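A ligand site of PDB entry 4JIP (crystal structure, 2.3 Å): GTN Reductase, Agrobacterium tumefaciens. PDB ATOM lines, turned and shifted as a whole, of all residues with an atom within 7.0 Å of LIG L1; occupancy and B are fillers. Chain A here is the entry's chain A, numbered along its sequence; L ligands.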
ATOM      1  N   PRO A  23      12.634   5.950  23.880  1.00  0.00           N
ATOM      2  CA  PRO A  23      13.702   6.268  22.915  1.00  0.00           C
ATOM      3  C   PRO A  23      14.789   7.124  23.551  1.00  0.00           C
ATOM      4  O   PRO A  23      14.478   8.130  24.193  1.00  0.00           O
ATOM      5  CB  PRO A  23      12.971   7.078  21.827  1.00  0.00           C
ATOM      6  CG  PRO A  23      11.725   7.607  22.507  1.00  0.00           C
ATOM      7  CD  PRO A  23      11.331   6.533  23.482  1.00  0.00           C
ATOM      8  N   LEU A  24      16.045   6.728  23.373  1.00  0.00           N
ATOM      9  CA  LEU A  24      17.164   7.428  24.003  1.00  0.00           C
ATOM     10  C   LEU A  24      18.384   7.592  23.083  1.00  0.00           C
ATOM     11  O   LEU A  24      19.182   6.669  22.923  1.00  0.00           O
ATOM     12  CB  LEU A  24      17.575   6.721  25.300  1.00  0.00           C
ATOM     13  CG  LEU A  24      16.528   6.582  26.411  1.00  0.00           C
ATOM     14  CD1 LEU A  24      16.852   5.377  27.278  1.00  0.00           C
ATOM     15  CD2 LEU A  24      16.422   7.846  27.261  1.00  0.00           C
ATOM     16  N   THR A  25      18.493   8.770  22.482  1.00  0.00           N
ATOM     17  CA  THR A  25      19.672   9.193  21.706  1.00  0.00           C
ATOM     18  C   THR A  25      20.940   9.038  22.549  1.00  0.00           C
ATOM     19  O   THR A  25      21.054   9.637  23.610  1.00  0.00           O
ATOM     20  CB  THR A  25      19.535  10.676  21.258  1.00  0.00           C
ATOM     21  OG1 THR A  25      18.405  10.816  20.396  1.00  0.00           O
ATOM     22  CG2 THR A  25      20.787  11.157  20.545  1.00  0.00           C
ATOM     23  N   ARG A  26      21.886   8.216  22.061  1.00  0.00           N
ATOM     24  CA  ARG A  26      23.122   7.907  22.792  1.00  0.00           C
ATOM     25  C   ARG A  26      24.390   8.315  22.006  1.00  0.00           C
ATOM     26  O   ARG A  26      25.508   8.284  22.550  1.00  0.00           O
ATOM     27  CB  ARG A  26      23.193   6.418  23.145  1.00  0.00           C
ATOM     28  CG  ARG A  26      21.972   5.858  23.870  1.00  0.00           C
ATOM     29  CD  ARG A  26      21.613   6.686  25.094  1.00  0.00           C
ATOM     30  NE  ARG A  26      22.756   6.819  25.998  1.00  0.00           N
ATOM     31  CZ  ARG A  26      23.103   5.928  26.921  1.00  0.00           C
ATOM     32  NH1 ARG A  26      24.165   6.129  27.692  1.00  0.00           N
ATOM     33  NH2 ARG A  26      22.381   4.821  27.079  1.00  0.00           N
ATOM     34  N   ASN A  27      24.211   8.669  20.737  1.00  0.00           N
ATOM     35  CA  ASN A  27      25.300   9.100  19.871  1.00  0.00           C
ATOM     36  C   ASN A  27      26.475   8.124  19.861  1.00  0.00           C
ATOM     37  O   ASN A  27      27.601   8.519  20.126  1.00  0.00           O
ATOM     38  CB  ASN A  27      25.813  10.479  20.286  1.00  0.00           C
ATOM     39  CG  ASN A  27      24.704  11.445  20.590  1.00  0.00           C
ATOM     40  OD1 ASN A  27      24.286  11.592  21.740  1.00  0.00           O
ATOM     41  ND2 ASN A  27      24.202  12.121  19.541  1.00  0.00           N
ATOM     42  N   GLY A  55      16.254   7.879  18.519  1.00  0.00           N
ATOM     43  CA  GLY A  55      15.844   8.511  17.276  1.00  0.00           C
ATOM     44  C   GLY A  55      16.726   8.030  16.132  1.00  0.00           C
ATOM     45  O   GLY A  55      17.954   8.068  16.222  1.00  0.00           O
ATOM     46  N   TYR A  65      21.988  15.293  15.106  1.00  0.00           N
ATOM     47  CA  TYR A  65      23.022  15.004  16.089  1.00  0.00           C
ATOM     48  C   TYR A  65      24.041  14.047  15.497  1.00  0.00           C
ATOM     49  O   TYR A  65      23.711  13.214  14.659  1.00  0.00           O
ATOM     50  CB  TYR A  65      22.413  14.427  17.374  1.00  0.00           C
ATOM     51  CG  TYR A  65      21.340  15.312  17.994  1.00  0.00           C
ATOM     52  CD1 TYR A  65      20.040  15.285  17.506  1.00  0.00           C
ATOM     53  CD2 TYR A  65      21.623  16.172  19.041  1.00  0.00           C
ATOM     54  CE1 TYR A  65      19.054  16.089  18.051  1.00  0.00           C
ATOM     55  CE2 TYR A  65      20.640  16.989  19.605  1.00  0.00           C
ATOM     56  CZ  TYR A  65      19.349  16.942  19.096  1.00  0.00           C
ATOM     57  OH  TYR A  65      18.360  17.733  19.624  1.00  0.00           O
ATOM     58  N   GLN A  97      12.211   4.363  16.164  1.00  0.00           N
ATOM     59  CA  GLN A  97      11.658   5.716  16.199  1.00  0.00           C
ATOM     60  C   GLN A  97      12.161   6.509  14.990  1.00  0.00           C
ATOM     61  O   GLN A  97      13.217   7.154  15.057  1.00  0.00           O
ATOM     62  CB  GLN A  97      11.992   6.456  17.504  1.00  0.00           C
ATOM     63  CG  GLN A  97      11.281   7.815  17.607  1.00  0.00           C
ATOM     64  CD  GLN A  97      11.711   8.676  18.788  1.00  0.00           C
ATOM     65  OE1 GLN A  97      12.897   8.827  19.070  1.00  0.00           O
ATOM     66  NE2 GLN A  97      10.728   9.263  19.481  1.00  0.00           N
ATOM     67  N   TRP A  99      12.799   9.361  12.505  1.00  0.00           N
ATOM     68  CA  TRP A  99      13.054  10.703  12.984  1.00  0.00           C
ATOM     69  C   TRP A  99      13.333  11.700  11.847  1.00  0.00           C
ATOM     70  O   TRP A  99      13.944  11.362  10.837  1.00  0.00           O
ATOM     71  CB  TRP A  99      14.281  10.635  13.906  1.00  0.00           C
ATOM     72  CG  TRP A  99      14.436  11.767  14.855  1.00  0.00           C
ATOM     73  CD1 TRP A  99      13.531  12.746  15.137  1.00  0.00           C
ATOM     74  CD2 TRP A  99      15.593  12.041  15.668  1.00  0.00           C
ATOM     75  NE1 TRP A  99      14.038  13.603  16.070  1.00  0.00           N
ATOM     76  CE2 TRP A  99      15.304  13.202  16.413  1.00  0.00           C
ATOM     77  CE3 TRP A  99      16.829  11.413  15.840  1.00  0.00           C
ATOM     78  CZ2 TRP A  99      16.217  13.750  17.324  1.00  0.00           C
ATOM     79  CZ3 TRP A  99      17.731  11.961  16.741  1.00  0.00           C
ATOM     80  CH2 TRP A  99      17.415  13.124  17.472  1.00  0.00           C
ATOM     81  N   PHE A 139      28.668  20.622  22.292  1.00  0.00           N
ATOM     82  CA  PHE A 139      27.343  21.130  22.037  1.00  0.00           C
ATOM     83  C   PHE A 139      27.468  22.453  21.304  1.00  0.00           C
ATOM     84  O   PHE A 139      28.282  23.304  21.692  1.00  0.00           O
ATOM     85  CB  PHE A 139      26.565  21.292  23.338  1.00  0.00           C
ATOM     86  CG  PHE A 139      26.008  20.006  23.865  1.00  0.00           C
ATOM     87  CD1 PHE A 139      24.830  19.504  23.343  1.00  0.00           C
ATOM     88  CD2 PHE A 139      26.660  19.297  24.851  1.00  0.00           C
ATOM     89  CE1 PHE A 139      24.304  18.307  23.807  1.00  0.00           C
ATOM     90  CE2 PHE A 139      26.144  18.099  25.325  1.00  0.00           C
ATOM     91  CZ  PHE A 139      24.961  17.605  24.799  1.00  0.00           C
ATOM     92  N   HIS A 178       8.341   9.786  15.326  1.00  0.00           N
ATOM     93  CA  HIS A 178       8.734  10.852  16.241  1.00  0.00           C
ATOM     94  C   HIS A 178       8.058  12.170  15.836  1.00  0.00           C
ATOM     95  O   HIS A 178       8.456  12.826  14.869  1.00  0.00           O
ATOM     96  CB  HIS A 178      10.269  11.016  16.278  1.00  0.00           C
ATOM     97  CG  HIS A 178      10.760  11.822  17.433  1.00  0.00           C
ATOM     98  ND1 HIS A 178       9.942  12.636  18.192  1.00  0.00           N
ATOM     99  CD2 HIS A 178      11.999  11.938  17.979  1.00  0.00           C
ATOM    100  CE1 HIS A 178      10.655  13.212  19.145  1.00  0.00           C
ATOM    101  NE2 HIS A 178      11.899  12.810  19.039  1.00  0.00           N
ATOM    102  N   ALA A 180       7.401  14.485  18.383  1.00  0.00           N
ATOM    103  CA  ALA A 180       7.471  15.124  19.672  1.00  0.00           C
ATOM    104  C   ALA A 180       8.698  16.015  19.811  1.00  0.00           C
ATOM    105  O   ALA A 180       9.486  16.144  18.878  1.00  0.00           O
ATOM    106  CB  ALA A 180       7.442  14.069  20.774  1.00  0.00           C
ATOM    107  N   ASN A 181       8.830  16.634  20.976  1.00  0.00           N
ATOM    108  CA  ASN A 181      10.054  17.292  21.398  1.00  0.00           C
ATOM    109  C   ASN A 181      10.621  18.370  20.441  1.00  0.00           C
ATOM    110  O   ASN A 181      11.835  18.510  20.295  1.00  0.00           O
ATOM    111  CB  ASN A 181      11.119  16.242  21.741  1.00  0.00           C
ATOM    112  CG  ASN A 181      10.658  15.314  22.856  1.00  0.00           C
ATOM    113  OD1 ASN A 181       9.842  15.703  23.705  1.00  0.00           O
ATOM    114  ND2 ASN A 181      11.182  14.092  22.871  1.00  0.00           N
ATOM    115  N   GLY A 182       9.734  19.120  19.804  1.00  0.00           N
ATOM    116  CA  GLY A 182      10.145  20.240  18.977  1.00  0.00           C
ATOM    117  C   GLY A 182      10.848  19.894  17.675  1.00  0.00           C
ATOM    118  O   GLY A 182      11.521  20.751  17.082  1.00  0.00           O
ATOM    119  N   TYR A 183      10.706  18.656  17.202  1.00  0.00           N
ATOM    120  CA  TYR A 183      11.312  18.282  15.914  1.00  0.00           C
ATOM    121  C   TYR A 183      10.387  18.613  14.745  1.00  0.00           C
ATOM    122  O   TYR A 183       9.383  19.302  14.939  1.00  0.00           O
ATOM    123  CB  TYR A 183      11.806  16.841  15.929  1.00  0.00           C
ATOM    124  CG  TYR A 183      12.904  16.704  16.944  1.00  0.00           C
ATOM    125  CD1 TYR A 183      14.162  17.248  16.710  1.00  0.00           C
ATOM    126  CD2 TYR A 183      12.674  16.097  18.168  1.00  0.00           C
ATOM    127  CE1 TYR A 183      15.157  17.160  17.652  1.00  0.00           C
ATOM    128  CE2 TYR A 183      13.666  16.002  19.121  1.00  0.00           C
ATOM    129  CZ  TYR A 183      14.906  16.542  18.855  1.00  0.00           C
ATOM    130  OH  TYR A 183      15.889  16.447  19.798  1.00  0.00           O
ATOM    131  N   ARG A 230       4.843   9.273  18.634  1.00  0.00           N
ATOM    132  CA  ARG A 230       5.073   9.931  19.915  1.00  0.00           C
ATOM    133  C   ARG A 230       4.648  11.397  19.843  1.00  0.00           C
ATOM    134  O   ARG A 230       4.999  12.100  18.917  1.00  0.00           O
ATOM    135  CB  ARG A 230       6.544   9.842  20.312  1.00  0.00           C
ATOM    136  CG  ARG A 230       6.809  10.326  21.732  1.00  0.00           C
ATOM    137  CD  ARG A 230       8.232  10.020  22.197  1.00  0.00           C
ATOM    138  NE  ARG A 230       8.243   9.525  23.572  1.00  0.00           N
ATOM    139  CZ  ARG A 230       9.225   9.742  24.434  1.00  0.00           C
ATOM    140  NH1 ARG A 230      10.288  10.441  24.069  1.00  0.00           N
ATOM    141  NH2 ARG A 230       9.166   9.253  25.668  1.00  0.00           N
ATOM    142  N   ALA A 237      10.888  21.580  25.011  1.00  0.00           N
ATOM    143  CA  ALA A 237      12.068  21.038  24.335  1.00  0.00           C
ATOM    144  C   ALA A 237      12.319  21.730  23.008  1.00  0.00           C
ATOM    145  O   ALA A 237      11.383  21.918  22.217  1.00  0.00           O
ATOM    146  CB  ALA A 237      11.919  19.519  24.094  1.00  0.00           C
ATOM    147  N   ASN A 238      13.571  22.117  22.787  1.00  0.00           N
ATOM    148  CA  ASN A 238      14.005  22.736  21.541  1.00  0.00           C
ATOM    149  C   ASN A 238      13.244  24.024  21.177  1.00  0.00           C
ATOM    150  O   ASN A 238      12.885  24.239  20.003  1.00  0.00           O
ATOM    151  CB  ASN A 238      13.965  21.694  20.415  1.00  0.00           C
ATOM    152  CG  ASN A 238      14.986  20.591  20.627  1.00  0.00           C
ATOM    153  OD1 ASN A 238      16.184  20.855  20.728  1.00  0.00           O
ATOM    154  ND2 ASN A 238      14.513  19.355  20.745  1.00  0.00           N
ATOM    155  N   THR A 271       9.564  17.574  28.654  1.00  0.00           N
ATOM    156  CA  THR A 271      10.366  16.373  28.425  1.00  0.00           C
ATOM    157  C   THR A 271      11.570  16.347  29.354  1.00  0.00           C
ATOM    158  O   THR A 271      12.462  17.184  29.252  1.00  0.00           O
ATOM    159  CB  THR A 271      10.847  16.263  26.956  1.00  0.00           C
ATOM    160  OG1 THR A 271       9.754  16.532  26.069  1.00  0.00           O
ATOM    161  CG2 THR A 271      11.422  14.863  26.685  1.00  0.00           C
ATOM    162  N   TYR A 356      25.593  10.845  26.271  1.00  0.00           N
ATOM    163  CA  TYR A 356      25.869  11.103  24.859  1.00  0.00           C
ATOM    164  C   TYR A 356      27.305  10.814  24.442  1.00  0.00           C
ATOM    165  O   TYR A 356      28.253  11.260  25.098  1.00  0.00           O
ATOM    166  CB  TYR A 356      25.554  12.571  24.557  1.00  0.00           C
ATOM    167  CG  TYR A 356      24.218  13.013  25.098  1.00  0.00           C
ATOM    168  CD1 TYR A 356      23.032  12.608  24.503  1.00  0.00           C
ATOM    169  CD2 TYR A 356      24.141  13.830  26.220  1.00  0.00           C
ATOM    170  CE1 TYR A 356      21.816  13.016  24.992  1.00  0.00           C
ATOM    171  CE2 TYR A 356      22.910  14.237  26.724  1.00  0.00           C
ATOM    172  CZ  TYR A 356      21.752  13.820  26.099  1.00  0.00           C
ATOM    173  OH  TYR A 356      20.526  14.215  26.577  1.00  0.00           O
HETATM  174  C1  LIG L   1      18.112  14.342  23.822  1.00  0.00           C
HETATM  175  O1  LIG L   1      19.230  14.162  23.332  1.00  0.00           O
HETATM  176  C2  LIG L   1      16.860  14.138  23.030  1.00  0.00           C
HETATM  177  C3  LIG L   1      16.878  13.778  21.689  1.00  0.00           C
HETATM  178  C4  LIG L   1      15.690  13.600  21.006  1.00  0.00           C
HETATM  179  C5  LIG L   1      14.476  13.763  21.640  1.00  0.00           C
HETATM  180  C6  LIG L   1      14.454  14.131  22.976  1.00  0.00           C
HETATM  181  C7  LIG L   1      15.640  14.300  23.671  1.00  0.00           C
HETATM  182  O2  LIG L   1      13.289  13.600  20.958  1.00  0.00           O
HETATM  183  N1  LG2 L   2      13.087  11.162  23.326  1.00  0.00           N
HETATM  184  C1  LG2 L   2      12.810  10.862  22.004  1.00  0.00           C
HETATM  185  O1  LG2 L   2      11.656  10.906  21.567  1.00  0.00           O
HETATM  186  N2  LG2 L   2      13.836  10.549  21.144  1.00  0.00           N
HETATM  187  C2  LG2 L   2      15.129  10.471  21.619  1.00  0.00           C
HETATM  188  O2  LG2 L   2      16.040  10.174  20.843  1.00  0.00           O
HETATM  189  C3  LG2 L   2      15.414  10.799  22.935  1.00  0.00           C
HETATM  190  N3  LG2 L   2      16.710  10.800  23.404  1.00  0.00           N
HETATM  191  C4  LG2 L   2      16.986  10.992  24.747  1.00  0.00           C
HETATM  192  C5  LG2 L   2      18.275  10.807  25.226  1.00  0.00           C
HETATM  193  C6  LG2 L   2      18.549  10.963  26.578  1.00  0.00           C
HETATM  194  C7  LG2 L   2      19.953  10.797  27.075  1.00  0.00           C
HETATM  195  C8  LG2 L   2      17.519  11.288  27.464  1.00  0.00           C
HETATM  196  C9  LG2 L   2      17.811  11.478  28.921  1.00  0.00           C
HETATM  197  C10 LG2 L   2      16.230  11.459  26.984  1.00  0.00           C
HETATM  198  C11 LG2 L   2      15.946  11.304  25.622  1.00  0.00           C
HETATM  199  N4  LG2 L   2      14.651  11.411  25.132  1.00  0.00           N
HETATM  200  C12 LG2 L   2      14.381  11.112  23.803  1.00  0.00           C
HETATM  201  C13 LG2 L   2      13.500  11.657  26.061  1.00  0.00           C
HETATM  202  C14 LG2 L   2      13.065  10.389  26.798  1.00  0.00           C
HETATM  203  O3  LG2 L   2      12.533   9.452  25.892  1.00  0.00           O
HETATM  204  C15 LG2 L   2      12.041  10.692  27.886  1.00  0.00           C
HETATM  205  O4  LG2 L   2      10.997  11.454  27.305  1.00  0.00           O
HETATM  206  C16 LG2 L   2      12.658  11.466  29.053  1.00  0.00           C
HETATM  207  O5  LG2 L   2      13.874  10.838  29.404  1.00  0.00           O
HETATM  208  C17 LG2 L   2      11.733  11.509  30.269  1.00  0.00           C
HETATM  209  O6  LG2 L   2      11.534  10.190  30.686  1.00  0.00           O
HETATM  210  P1  LG2 L   2      12.131   9.621  32.080  1.00  0.00           P
HETATM  211  O7  LG2 L   2      11.620   8.214  32.220  1.00  0.00           O
HETATM  212  O8  LG2 L   2      13.644   9.630  32.014  1.00  0.00           O
HETATM  213  O9  LG2 L   2      11.664  10.478  33.224  1.00  0.00           O
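An oxygen (O2) of LIG L1 is in hydrogen-bond range of a ring nitrogen (NE2) of His 178. An oxygen (O2) of LIG L1 lies within hydrogen-bond range of the side-chain amide nitrogen (ND2) of Asn 181, 2.9 Å away. An oxygen (O1) of LIG L1 sits close to the side-chain hydroxyl (OH) of Tyr 356. NE2 of His 178 sits at hydrogen-bond distance from O1 of LG2 L2. The side-chain amide nitrogen of Asn 181 lies within hydrogen-bond range of an oxygen (O1) of LG2 L2, 3.5 Å away. The backbone NH (N) of Thr 25 is in hydrogen-bond range of a nitrogen (N3) of LG2 L2 (2.9 Å). O2 of LG2 L2 sits at hydrogen-bond distance from OG1 of Thr 25, at 2.5 Å. The side-chain amide nitrogen (NE2) of Gln 97 lies within hydrogen-bond range of an oxygen (O1) of LG2 L2 (2.8 Å). NH1 of Arg 230 lies within hydrogen-bond range of O1 of LG2 L2, 2.9 Å away. The backbone carbonyl oxygen of Pro 23 sits at hydrogen-bond distance from an oxygen (O3) of LG2 L2 (2.9 Å). The backbone NH (N) of Gly 55 is in hydrogen-bond range of an oxygen (O2) of LG2 L2.
O2 of LIG L1 sits close to N2 of LG2 L2.
A ring nitrogen (ND1) of His 178 sits at hydrogen-bond distance from the backbone NH of Ala 180. OG1 of Thr 271 is in hydrogen-bond range of OD1 of Asn 181, 2.5 Å away. The backbone carbonyl oxygen (O) of Asn 181 is in hydrogen-bond range of the side-chain amide nitrogen (ND2) of Asn 238 (2.8 Å). The side-chain hydroxyl (OH) of Tyr 183 sits at hydrogen-bond distance from the side-chain hydroxyl (OH) of Tyr 65 (2.8 Å). The side-chain hydroxyl (OH) of Tyr 183 is in hydrogen-bond range of the side-chain amide nitrogen (ND2) of Asn 238 (3.4 Å).
OG1 of Thr 25 touches C3 of LIG L1 (3.6 Å). Trp 99 touches LIG L1. Tyr 183 touches LIG L1. Six residues have an atom within 4 Å of LIG L1: Thr 25, Trp 99, His 178, Asn 181, Tyr 183 and Tyr 356. The nearest printed residue that does not touch LIG L1 is Tyr 65 (4.7 Å).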
